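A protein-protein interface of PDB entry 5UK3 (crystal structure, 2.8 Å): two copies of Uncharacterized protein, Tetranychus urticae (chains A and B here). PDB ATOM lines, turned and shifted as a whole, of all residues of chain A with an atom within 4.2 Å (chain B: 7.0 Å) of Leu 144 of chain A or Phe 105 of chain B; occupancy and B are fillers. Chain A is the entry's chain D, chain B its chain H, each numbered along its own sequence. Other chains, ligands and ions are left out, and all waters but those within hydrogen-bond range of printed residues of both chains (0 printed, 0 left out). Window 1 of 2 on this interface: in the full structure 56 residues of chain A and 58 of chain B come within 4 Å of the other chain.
The backbone carbonyl oxygen of Leu 144 of chain A is in hydrogen-bond range of the backbone NH of Ile 146 of chain B. The backbone NH (N) of Ile 146 of chain A is in hydrogen-bond range of the backbone carbonyl oxygen (O) of Leu 144 of chain B. The backbone carbonyl oxygen of Gly 148 of chain B sits at hydrogen-bond distance from the backbone NH of Val 142 of chain A (2.8 Å).
The backbone carbonyl oxygen of Asp 133 of chain A is in hydrogen-bond range of the backbone NH of Arg 145 of chain A. The guanidinium group (NH1) of Arg 145 of chain B lies within salt-bridge range of the side-chain carboxylate (OD2) of Asp 147 of chain B (3.8 Å).
CG of Phe 101 of chain A touches CE1 of Phe 105 of chain B, at 3.6 Å. Phe 105 of chain A touches Phe 101 of chain B. Phe 105 of chain A touches Leu 144 of chain B. Leu 104 of chain B touches Ile 132 of chain A. Val 142 of chain A touches Met 125 of chain B. Ile 146 of chain B touches Val 142 of chain A (O to O, 3.7 Å). CA of Asp 147 of chain B touches O of Val 142 of chain A (3.6 Å). Ile 143 of chain A touches Arg 145 of chain B. Phe 105 of chain B touches Leu 144 of chain A (CE1 to CD2, 3.98 Å). Arg 145 of chain A touches Leu 144 of chain B (CA to O, 3.7 Å).
Of the printed residues of chain B, Ile 132 of chain A touches Leu 104 (3.8 Å). Of chain B, only Phe 105, Leu 112, Leu 144, Arg 145 and Ile 146 come within 4 Å of Leu 144 of chain A. Of the printed residues of chain B, Ile 146 of chain A touches Leu 104 (3.7 Å) and Leu 144 (2.8 Å). Printed residues of chain A within 4 Å of Phe 101 of chain B: Phe 105 (3.5 Å). Glu 103 of chain B touches none of the printed residues of chain A. Phe 105 of chain B touches just these residues of chain A: Phe 101 (3.6 Å), Phe 105 (3.4 Å) and Leu 144 (3.98 Å). Ser 110 of chain B touches none of the printed residues of chain A. Of the printed residues of chain A, Asp 147 of chain B touches Val 142. The nearest residue of chain A that does not touch Phe 105 of chain B is Ile 146 of chain A (4.1 Å).
Printed residues of chain A that touch a printed residue of chain B: Phe 101, Phe 105, Ile 132, Val 142, Ile 143, Leu 144, Arg 145 and Ile 146. Hydrophobic or aromatic side chains of chain A within 4 Å of the printed part of chain B: Phe 101, Phe 105, Ile 132, Val 142, Ile 143, Leu 144 and Ile 146. Hydrophobic or aromatic side chains of chain B within 4 Å of the printed part of chain A: Phe 101, Leu 104, Phe 105, Leu 112, Met 125, Leu 144 and Ile 146. Among the printed residues, 20 pairs touch across the chains. Among the printed residues, no Asp or Glu carboxylate lies within 4 Å of a Lys or Arg side-chain nitrogen of the other chain.
Phe 101 of chain A touches Phe 105 of chain B, and with the chains exchanged Phe 105 of chain A touches Phe 101 of chain B. Phe 105 of chain A touches its own counterpart, Phe 105 of chain B. Phe 105 of chain A touches Leu 144 of chain B, and with the chains exchanged Leu 144 of chain A touches Phe 105 of chain B. Leu 144 of chain A touches Arg 145 of chain B, and with the chains exchanged Arg 145 of chain A touches Leu 144 of chain B. Positions printed for both chains: 101, 105, 144, 145 and 146. Of the 20 pairs that touch across the chains among the printed residues, 10 have their exchanged pair printed and touching as well.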
ATOM      1  N   PHE A 101      30.777 -29.972  19.300  1.00  0.00           N
ATOM      2  CA  PHE A 101      30.808 -28.749  20.088  1.00  0.00           C
ATOM      3  C   PHE A 101      32.220 -28.433  20.529  1.00  0.00           C
ATOM      4  O   PHE A 101      32.619 -27.300  20.509  1.00  0.00           O
ATOM      5  CB  PHE A 101      29.852 -28.814  21.267  1.00  0.00           C
ATOM      6  CG  PHE A 101      28.426 -28.866  20.852  1.00  0.00           C
ATOM      7  CD1 PHE A 101      27.894 -27.854  20.083  1.00  0.00           C
ATOM      8  CD2 PHE A 101      27.613 -29.920  21.218  1.00  0.00           C
ATOM      9  CE1 PHE A 101      26.579 -27.890  19.676  1.00  0.00           C
ATOM     10  CE2 PHE A 101      26.280 -29.962  20.834  1.00  0.00           C
ATOM     11  CZ  PHE A 101      25.767 -28.942  20.055  1.00  0.00           C
ATOM     12  N   PHE A 105      34.791 -24.979  19.431  1.00  0.00           N
ATOM     13  CA  PHE A 105      35.597 -24.022  20.221  1.00  0.00           C
ATOM     14  C   PHE A 105      37.089 -24.156  20.028  1.00  0.00           C
ATOM     15  O   PHE A 105      37.844 -23.268  20.367  1.00  0.00           O
ATOM     16  CB  PHE A 105      35.215 -24.073  21.693  1.00  0.00           C
ATOM     17  CG  PHE A 105      33.844 -23.575  21.931  1.00  0.00           C
ATOM     18  CD1 PHE A 105      33.594 -22.212  22.040  1.00  0.00           C
ATOM     19  CD2 PHE A 105      32.778 -24.461  21.931  1.00  0.00           C
ATOM     20  CE1 PHE A 105      32.291 -21.749  22.216  1.00  0.00           C
ATOM     21  CE2 PHE A 105      31.480 -24.009  22.103  1.00  0.00           C
ATOM     22  CZ  PHE A 105      31.233 -22.656  22.249  1.00  0.00           C
ATOM     23  N   ILE A 132      21.283 -22.033  28.823  1.00  0.00           N
ATOM     24  CA  ILE A 132      21.325 -22.648  27.502  1.00  0.00           C
ATOM     25  C   ILE A 132      19.894 -22.764  27.019  1.00  0.00           C
ATOM     26  O   ILE A 132      18.975 -22.939  27.798  1.00  0.00           O
ATOM     27  CB  ILE A 132      21.913 -24.061  27.504  1.00  0.00           C
ATOM     28  CG1 ILE A 132      23.154 -24.203  28.404  1.00  0.00           C
ATOM     29  CG2 ILE A 132      22.252 -24.489  26.082  1.00  0.00           C
ATOM     30  CD1 ILE A 132      24.235 -23.233  28.080  1.00  0.00           C
ATOM     31  N   ASP A 133      19.718 -22.671  25.723  1.00  0.00           N
ATOM     32  CA  ASP A 133      18.442 -22.910  25.091  1.00  0.00           C
ATOM     33  C   ASP A 133      18.725 -23.635  23.786  1.00  0.00           C
ATOM     34  O   ASP A 133      19.726 -23.342  23.139  1.00  0.00           O
ATOM     35  CB  ASP A 133      17.798 -21.571  24.823  1.00  0.00           C
ATOM     36  CG  ASP A 133      16.430 -21.702  24.256  1.00  0.00           C
ATOM     37  OD1 ASP A 133      15.976 -22.871  24.091  1.00  0.00           O
ATOM     38  OD2 ASP A 133      15.783 -20.647  24.002  1.00  0.00           O
ATOM     39  N   VAL A 134      17.899 -24.596  23.404  1.00  0.00           N
ATOM     40  CA  VAL A 134      18.162 -25.322  22.167  1.00  0.00           C
ATOM     41  C   VAL A 134      16.861 -25.609  21.459  1.00  0.00           C
ATOM     42  O   VAL A 134      15.903 -26.004  22.071  1.00  0.00           O
ATOM     43  CB  VAL A 134      19.025 -26.591  22.395  1.00  0.00           C
ATOM     44  CG1 VAL A 134      18.324 -27.589  23.272  1.00  0.00           C
ATOM     45  CG2 VAL A 134      19.411 -27.252  21.083  1.00  0.00           C
ATOM     46  N   VAL A 142      19.741 -26.701  13.960  1.00  0.00           N
ATOM     47  CA  VAL A 142      19.861 -26.783  15.403  1.00  0.00           C
ATOM     48  C   VAL A 142      20.280 -25.419  15.831  1.00  0.00           C
ATOM     49  O   VAL A 142      21.298 -24.928  15.377  1.00  0.00           O
ATOM     50  CB  VAL A 142      20.938 -27.789  15.861  1.00  0.00           C
ATOM     51  CG1 VAL A 142      20.913 -27.935  17.373  1.00  0.00           C
ATOM     52  CG2 VAL A 142      20.716 -29.150  15.240  1.00  0.00           C
ATOM     53  N   ILE A 143      19.519 -24.810  16.718  1.00  0.00           N
ATOM     54  CA  ILE A 143      19.842 -23.474  17.162  1.00  0.00           C
ATOM     55  C   ILE A 143      20.075 -23.487  18.629  1.00  0.00           C
ATOM     56  O   ILE A 143      19.155 -23.719  19.409  1.00  0.00           O
ATOM     57  CB  ILE A 143      18.757 -22.516  16.743  1.00  0.00           C
ATOM     58  CG1 ILE A 143      18.916 -22.400  15.227  1.00  0.00           C
ATOM     59  CG2 ILE A 143      18.898 -21.179  17.434  1.00  0.00           C
ATOM     60  CD1 ILE A 143      17.907 -21.584  14.524  1.00  0.00           C
ATOM     61  N   LEU A 144      21.321 -23.204  18.989  1.00  0.00           N
ATOM     62  CA  LEU A 144      21.797 -23.340  20.334  1.00  0.00           C
ATOM     63  C   LEU A 144      22.130 -21.954  20.807  1.00  0.00           C
ATOM     64  O   LEU A 144      22.980 -21.318  20.248  1.00  0.00           O
ATOM     65  CB  LEU A 144      23.023 -24.250  20.312  1.00  0.00           C
ATOM     66  CG  LEU A 144      23.797 -24.502  21.607  1.00  0.00           C
ATOM     67  CD1 LEU A 144      22.841 -25.185  22.550  1.00  0.00           C
ATOM     68  CD2 LEU A 144      25.043 -25.357  21.541  1.00  0.00           C
ATOM     69  N   ARG A 145      21.428 -21.468  21.817  1.00  0.00           N
ATOM     70  CA  ARG A 145      21.644 -20.119  22.325  1.00  0.00           C
ATOM     71  C   ARG A 145      22.201 -20.207  23.737  1.00  0.00           C
ATOM     72  O   ARG A 145      21.566 -20.800  24.595  1.00  0.00           O
ATOM     73  CB  ARG A 145      20.326 -19.367  22.314  1.00  0.00           C
ATOM     74  CG  ARG A 145      20.366 -17.976  22.894  1.00  0.00           C
ATOM     75  CD  ARG A 145      19.015 -17.315  22.732  1.00  0.00           C
ATOM     76  NE  ARG A 145      19.061 -15.860  22.942  1.00  0.00           N
ATOM     77  CZ  ARG A 145      19.099 -15.241  24.134  1.00  0.00           C
ATOM     78  NH1 ARG A 145      19.129 -15.923  25.278  1.00  0.00           N
ATOM     79  NH2 ARG A 145      19.109 -13.907  24.180  1.00  0.00           N
ATOM     80  N   ILE A 146      23.348 -19.589  23.993  1.00  0.00           N
ATOM     81  CA  ILE A 146      23.972 -19.588  25.308  1.00  0.00           C
ATOM     82  C   ILE A 146      23.993 -18.161  25.836  1.00  0.00           C
ATOM     83  O   ILE A 146      24.440 -17.272  25.154  1.00  0.00           O
ATOM     84  CB  ILE A 146      25.398 -20.142  25.209  1.00  0.00           C
ATOM     85  CG1 ILE A 146      25.359 -21.573  24.658  1.00  0.00           C
ATOM     86  CG2 ILE A 146      26.080 -20.128  26.566  1.00  0.00           C
ATOM     87  CD1 ILE A 146      26.718 -22.181  24.369  1.00  0.00           C
ATOM     88  N   TYR B  99      38.304 -22.211  28.671  1.00  0.00           N
ATOM     89  CA  TYR B  99      37.974 -23.350  29.559  1.00  0.00           C
ATOM     90  C   TYR B  99      36.508 -23.359  29.884  1.00  0.00           C
ATOM     91  O   TYR B  99      35.880 -24.387  29.883  1.00  0.00           O
ATOM     92  CB  TYR B  99      38.789 -23.355  30.865  1.00  0.00           C
ATOM     93  CG  TYR B  99      38.441 -24.532  31.713  1.00  0.00           C
ATOM     94  CD1 TYR B  99      38.938 -25.787  31.429  1.00  0.00           C
ATOM     95  CD2 TYR B  99      37.510 -24.415  32.704  1.00  0.00           C
ATOM     96  CE1 TYR B  99      38.552 -26.901  32.155  1.00  0.00           C
ATOM     97  CE2 TYR B  99      37.112 -25.505  33.422  1.00  0.00           C
ATOM     98  CZ  TYR B  99      37.641 -26.751  33.160  1.00  0.00           C
ATOM     99  OH  TYR B  99      37.249 -27.823  33.965  1.00  0.00           O
ATOM    100  N   ARG B 100      35.938 -22.197  30.162  1.00  0.00           N
ATOM    101  CA  ARG B 100      34.538 -22.178  30.548  1.00  0.00           C
ATOM    102  C   ARG B 100      33.654 -22.762  29.477  1.00  0.00           C
ATOM    103  O   ARG B 100      32.770 -23.553  29.774  1.00  0.00           O
ATOM    104  CB  ARG B 100      34.076 -20.775  30.912  1.00  0.00           C
ATOM    105  CG  ARG B 100      34.204 -20.458  32.388  1.00  0.00           C
ATOM    106  CD  ARG B 100      35.531 -19.804  32.681  1.00  0.00           C
ATOM    107  NE  ARG B 100      35.698 -19.528  34.099  1.00  0.00           N
ATOM    108  CZ  ARG B 100      36.769 -19.870  34.796  1.00  0.00           C
ATOM    109  NH1 ARG B 100      37.770 -20.495  34.208  1.00  0.00           N
ATOM    110  NH2 ARG B 100      36.847 -19.575  36.081  1.00  0.00           N
ATOM    111  N   PHE B 101      33.887 -22.416  28.223  1.00  0.00           N
ATOM    112  CA  PHE B 101      33.061 -23.051  27.176  1.00  0.00           C
ATOM    113  C   PHE B 101      33.200 -24.548  27.211  1.00  0.00           C
ATOM    114  O   PHE B 101      32.223 -25.243  27.083  1.00  0.00           O
ATOM    115  CB  PHE B 101      33.377 -22.498  25.790  1.00  0.00           C
ATOM    116  CG  PHE B 101      32.983 -21.049  25.621  1.00  0.00           C
ATOM    117  CD1 PHE B 101      31.666 -20.662  25.788  1.00  0.00           C
ATOM    118  CD2 PHE B 101      33.927 -20.083  25.305  1.00  0.00           C
ATOM    119  CE1 PHE B 101      31.300 -19.347  25.648  1.00  0.00           C
ATOM    120  CE2 PHE B 101      33.574 -18.759  25.170  1.00  0.00           C
ATOM    121  CZ  PHE B 101      32.253 -18.395  25.348  1.00  0.00           C
ATOM    122  N   ASN B 102      34.401 -25.042  27.460  1.00  0.00           N
ATOM    123  CA  ASN B 102      34.597 -26.483  27.558  1.00  0.00           C
ATOM    124  C   ASN B 102      33.876 -27.089  28.765  1.00  0.00           C
ATOM    125  O   ASN B 102      33.205 -28.135  28.647  1.00  0.00           O
ATOM    126  CB  ASN B 102      36.083 -26.827  27.395  1.00  0.00           C
ATOM    127  CG  ASN B 102      36.575 -26.562  25.952  1.00  0.00           C
ATOM    128  OD1 ASN B 102      35.852 -26.783  24.941  1.00  0.00           O
ATOM    129  ND2 ASN B 102      37.815 -26.070  25.847  1.00  0.00           N
ATOM    130  N   GLU B 103      33.900 -26.376  29.881  1.00  0.00           N
ATOM    131  CA  GLU B 103      33.247 -26.849  31.089  1.00  0.00           C
ATOM    132  C   GLU B 103      31.753 -26.901  30.868  1.00  0.00           C
ATOM    133  O   GLU B 103      31.053 -27.817  31.328  1.00  0.00           O
ATOM    134  CB  GLU B 103      33.561 -25.926  32.253  1.00  0.00           C
ATOM    135  CG  GLU B 103      32.693 -26.171  33.468  1.00  0.00           C
ATOM    136  CD  GLU B 103      33.286 -25.563  34.712  1.00  0.00           C
ATOM    137  OE1 GLU B 103      32.759 -24.489  35.135  1.00  0.00           O
ATOM    138  OE2 GLU B 103      34.303 -26.145  35.209  1.00  0.00           O
ATOM    139  N   LEU B 104      31.266 -25.901  30.158  1.00  0.00           N
ATOM    140  CA  LEU B 104      29.880 -25.840  29.873  1.00  0.00           C
ATOM    141  C   LEU B 104      29.380 -27.096  29.189  1.00  0.00           C
ATOM    142  O   LEU B 104      28.330 -27.584  29.535  1.00  0.00           O
ATOM    143  CB  LEU B 104      29.592 -24.590  29.069  1.00  0.00           C
ATOM    144  CG  LEU B 104      28.140 -24.234  28.810  1.00  0.00           C
ATOM    145  CD1 LEU B 104      27.483 -23.956  30.146  1.00  0.00           C
ATOM    146  CD2 LEU B 104      28.022 -22.992  27.947  1.00  0.00           C
ATOM    147  N   PHE B 105      30.111 -27.634  28.215  1.00  0.00           N
ATOM    148  CA  PHE B 105      29.657 -28.861  27.541  1.00  0.00           C
ATOM    149  C   PHE B 105      29.993 -30.102  28.324  1.00  0.00           C
ATOM    150  O   PHE B 105      29.467 -31.172  28.045  1.00  0.00           O
ATOM    151  CB  PHE B 105      30.167 -28.919  26.120  1.00  0.00           C
ATOM    152  CG  PHE B 105      29.563 -27.886  25.268  1.00  0.00           C
ATOM    153  CD1 PHE B 105      28.334 -28.082  24.700  1.00  0.00           C
ATOM    154  CD2 PHE B 105      30.177 -26.682  25.080  1.00  0.00           C
ATOM    155  CE1 PHE B 105      27.738 -27.088  23.899  1.00  0.00           C
ATOM    156  CE2 PHE B 105      29.588 -25.682  24.308  1.00  0.00           C
ATOM    157  CZ  PHE B 105      28.372 -25.885  23.708  1.00  0.00           C
ATOM    158  N   LYS B 106      30.908 -30.006  29.283  1.00  0.00           N
ATOM    159  CA  LYS B 106      31.100 -31.118  30.221  1.00  0.00           C
ATOM    160  C   LYS B 106      29.873 -31.271  31.129  1.00  0.00           C
ATOM    161  O   LYS B 106      29.434 -32.383  31.394  1.00  0.00           O
ATOM    162  CB  LYS B 106      32.379 -30.958  31.036  1.00  0.00           C
ATOM    163  CG  LYS B 106      33.561 -31.668  30.402  1.00  0.00           C
ATOM    164  CD  LYS B 106      34.813 -31.621  31.274  1.00  0.00           C
ATOM    165  CE  LYS B 106      35.769 -30.520  30.843  1.00  0.00           C
ATOM    166  NZ  LYS B 106      36.790 -30.257  31.890  1.00  0.00           N
ATOM    167  N   VAL B 107      29.299 -30.160  31.548  1.00  0.00           N
ATOM    168  CA  VAL B 107      28.158 -30.185  32.426  1.00  0.00           C
ATOM    169  C   VAL B 107      26.844 -30.443  31.690  1.00  0.00           C
ATOM    170  O   VAL B 107      26.047 -31.267  32.147  1.00  0.00           O
ATOM    171  CB  VAL B 107      28.072 -28.883  33.235  1.00  0.00           C
ATOM    172  CG1 VAL B 107      26.762 -28.777  33.989  1.00  0.00           C
ATOM    173  CG2 VAL B 107      29.220 -28.822  34.226  1.00  0.00           C
ATOM    174  N   TYR B 108      26.595 -29.724  30.592  1.00  0.00           N
ATOM    175  CA  TYR B 108      25.313 -29.837  29.885  1.00  0.00           C
ATOM    176  C   TYR B 108      25.355 -30.754  28.659  1.00  0.00           C
ATOM    177  O   TYR B 108      24.343 -30.917  27.962  1.00  0.00           O
ATOM    178  CB  TYR B 108      24.801 -28.464  29.484  1.00  0.00           C
ATOM    179  CG  TYR B 108      24.472 -27.623  30.657  1.00  0.00           C
ATOM    180  CD1 TYR B 108      23.274 -27.767  31.341  1.00  0.00           C
ATOM    181  CD2 TYR B 108      25.374 -26.700  31.129  1.00  0.00           C
ATOM    182  CE1 TYR B 108      22.982 -26.984  32.463  1.00  0.00           C
ATOM    183  CE2 TYR B 108      25.097 -25.911  32.245  1.00  0.00           C
ATOM    184  CZ  TYR B 108      23.900 -26.045  32.909  1.00  0.00           C
ATOM    185  OH  TYR B 108      23.674 -25.240  33.997  1.00  0.00           O
ATOM    186  N   GLY B 109      26.496 -31.389  28.398  1.00  0.00           N
ATOM    187  CA  GLY B 109      26.645 -32.182  27.194  1.00  0.00           C
ATOM    188  C   GLY B 109      25.607 -33.261  27.054  1.00  0.00           C
ATOM    189  O   GLY B 109      24.927 -33.327  26.040  1.00  0.00           O
ATOM    190  N   SER B 110      25.450 -34.080  28.075  1.00  0.00           N
ATOM    191  CA  SER B 110      24.502 -35.174  27.982  1.00  0.00           C
ATOM    192  C   SER B 110      23.076 -34.697  27.834  1.00  0.00           C
ATOM    193  O   SER B 110      22.271 -35.380  27.206  1.00  0.00           O
ATOM    194  CB  SER B 110      24.603 -36.110  29.197  1.00  0.00           C
ATOM    195  OG  SER B 110      24.154 -35.487  30.378  1.00  0.00           O
ATOM    196  N   LEU B 112      22.138 -31.818  26.274  1.00  0.00           N
ATOM    197  CA  LEU B 112      22.012 -31.369  24.890  1.00  0.00           C
ATOM    198  C   LEU B 112      21.901 -32.550  23.954  1.00  0.00           C
ATOM    199  O   LEU B 112      21.149 -32.530  22.987  1.00  0.00           O
ATOM    200  CB  LEU B 112      23.202 -30.499  24.499  1.00  0.00           C
ATOM    201  CG  LEU B 112      23.208 -29.153  25.216  1.00  0.00           C
ATOM    202  CD1 LEU B 112      24.548 -28.461  25.018  1.00  0.00           C
ATOM    203  CD2 LEU B 112      22.087 -28.268  24.740  1.00  0.00           C
ATOM    204  N   ILE B 116      18.571 -33.050  21.715  1.00  0.00           N
ATOM    205  CA  ILE B 116      18.723 -33.078  20.268  1.00  0.00           C
ATOM    206  C   ILE B 116      18.223 -34.394  19.720  1.00  0.00           C
ATOM    207  O   ILE B 116      17.567 -34.409  18.673  1.00  0.00           O
ATOM    208  CB  ILE B 116      20.166 -32.798  19.812  1.00  0.00           C
ATOM    209  CG1 ILE B 116      20.511 -31.321  20.044  1.00  0.00           C
ATOM    210  CG2 ILE B 116      20.330 -33.069  18.327  1.00  0.00           C
ATOM    211  CD1 ILE B 116      21.996 -31.028  20.048  1.00  0.00           C
ATOM    212  N   MET B 125      24.860 -32.097  15.324  1.00  0.00           N
ATOM    213  CA  MET B 125      24.879 -30.733  14.824  1.00  0.00           C
ATOM    214  C   MET B 125      26.256 -30.478  14.279  1.00  0.00           C
ATOM    215  O   MET B 125      27.227 -30.667  14.999  1.00  0.00           O
ATOM    216  CB  MET B 125      24.601 -29.745  15.928  1.00  0.00           C
ATOM    217  CG  MET B 125      24.527 -28.324  15.403  1.00  0.00           C
ATOM    218  SD  MET B 125      24.771 -27.084  16.672  1.00  0.00           S
ATOM    219  CE  MET B 125      26.569 -26.986  16.577  1.00  0.00           C
ATOM    220  N   LEU B 144      25.725 -15.807  23.021  1.00  0.00           N
ATOM    221  CA  LEU B 144      26.427 -16.576  22.035  1.00  0.00           C
ATOM    222  C   LEU B 144      25.402 -17.437  21.347  1.00  0.00           C
ATOM    223  O   LEU B 144      24.765 -18.249  21.985  1.00  0.00           O
ATOM    224  CB  LEU B 144      27.476 -17.424  22.756  1.00  0.00           C
ATOM    225  CG  LEU B 144      28.332 -18.409  21.966  1.00  0.00           C
ATOM    226  CD1 LEU B 144      29.122 -17.597  20.993  1.00  0.00           C
ATOM    227  CD2 LEU B 144      29.333 -19.261  22.741  1.00  0.00           C
ATOM    228  N   ARG B 145      25.200 -17.226  20.058  1.00  0.00           N
ATOM    229  CA  ARG B 145      24.188 -17.977  19.315  1.00  0.00           C
ATOM    230  C   ARG B 145      24.885 -18.847  18.280  1.00  0.00           C
ATOM    231  O   ARG B 145      25.629 -18.335  17.475  1.00  0.00           O
ATOM    232  CB  ARG B 145      23.242 -16.999  18.633  1.00  0.00           C
ATOM    233  CG  ARG B 145      22.190 -17.617  17.729  1.00  0.00           C
ATOM    234  CD  ARG B 145      21.285 -16.520  17.183  1.00  0.00           C
ATOM    235  NE  ARG B 145      20.039 -17.038  16.597  1.00  0.00           N
ATOM    236  CZ  ARG B 145      19.919 -17.612  15.395  1.00  0.00           C
ATOM    237  NH1 ARG B 145      20.971 -17.770  14.590  1.00  0.00           N
ATOM    238  NH2 ARG B 145      18.730 -18.041  14.993  1.00  0.00           N
ATOM    239  N   ILE B 146      24.628 -20.144  18.304  1.00  0.00           N
ATOM    240  CA  ILE B 146      25.247 -21.099  17.388  1.00  0.00           C
ATOM    241  C   ILE B 146      24.155 -21.710  16.531  1.00  0.00           C
ATOM    242  O   ILE B 146      23.162 -22.183  17.054  1.00  0.00           O
ATOM    243  CB  ILE B 146      25.972 -22.193  18.169  1.00  0.00           C
ATOM    244  CG1 ILE B 146      27.066 -21.559  19.046  1.00  0.00           C
ATOM    245  CG2 ILE B 146      26.587 -23.199  17.217  1.00  0.00           C
ATOM    246  CD1 ILE B 146      27.767 -22.524  19.988  1.00  0.00           C
ATOM    247  N   ASP B 147      24.331 -21.683  15.215  1.00  0.00           N
ATOM    248  CA  ASP B 147      23.273 -22.084  14.254  1.00  0.00           C
ATOM    249  C   ASP B 147      23.835 -23.122  13.262  1.00  0.00           C
ATOM    250  O   ASP B 147      24.536 -22.758  12.318  1.00  0.00           O
ATOM    251  CB  ASP B 147      22.752 -20.836  13.516  1.00  0.00           C
ATOM    252  CG  ASP B 147      21.800 -21.165  12.339  1.00  0.00           C
ATOM    253  OD1 ASP B 147      21.511 -22.374  12.125  1.00  0.00           O
ATOM    254  OD2 ASP B 147      21.333 -20.213  11.651  1.00  0.00           O
ATOM    255  N   GLY B 148      23.535 -24.404  13.497  1.00  0.00           N
ATOM    256  CA  GLY B 148      24.221 -25.517  12.808  1.00  0.00           C
ATOM    257  C   GLY B 148      23.276 -26.452  12.104  1.00  0.00           C
ATOM    258  O   GLY B 148      22.122 -26.519  12.474  1.00  0.00           O
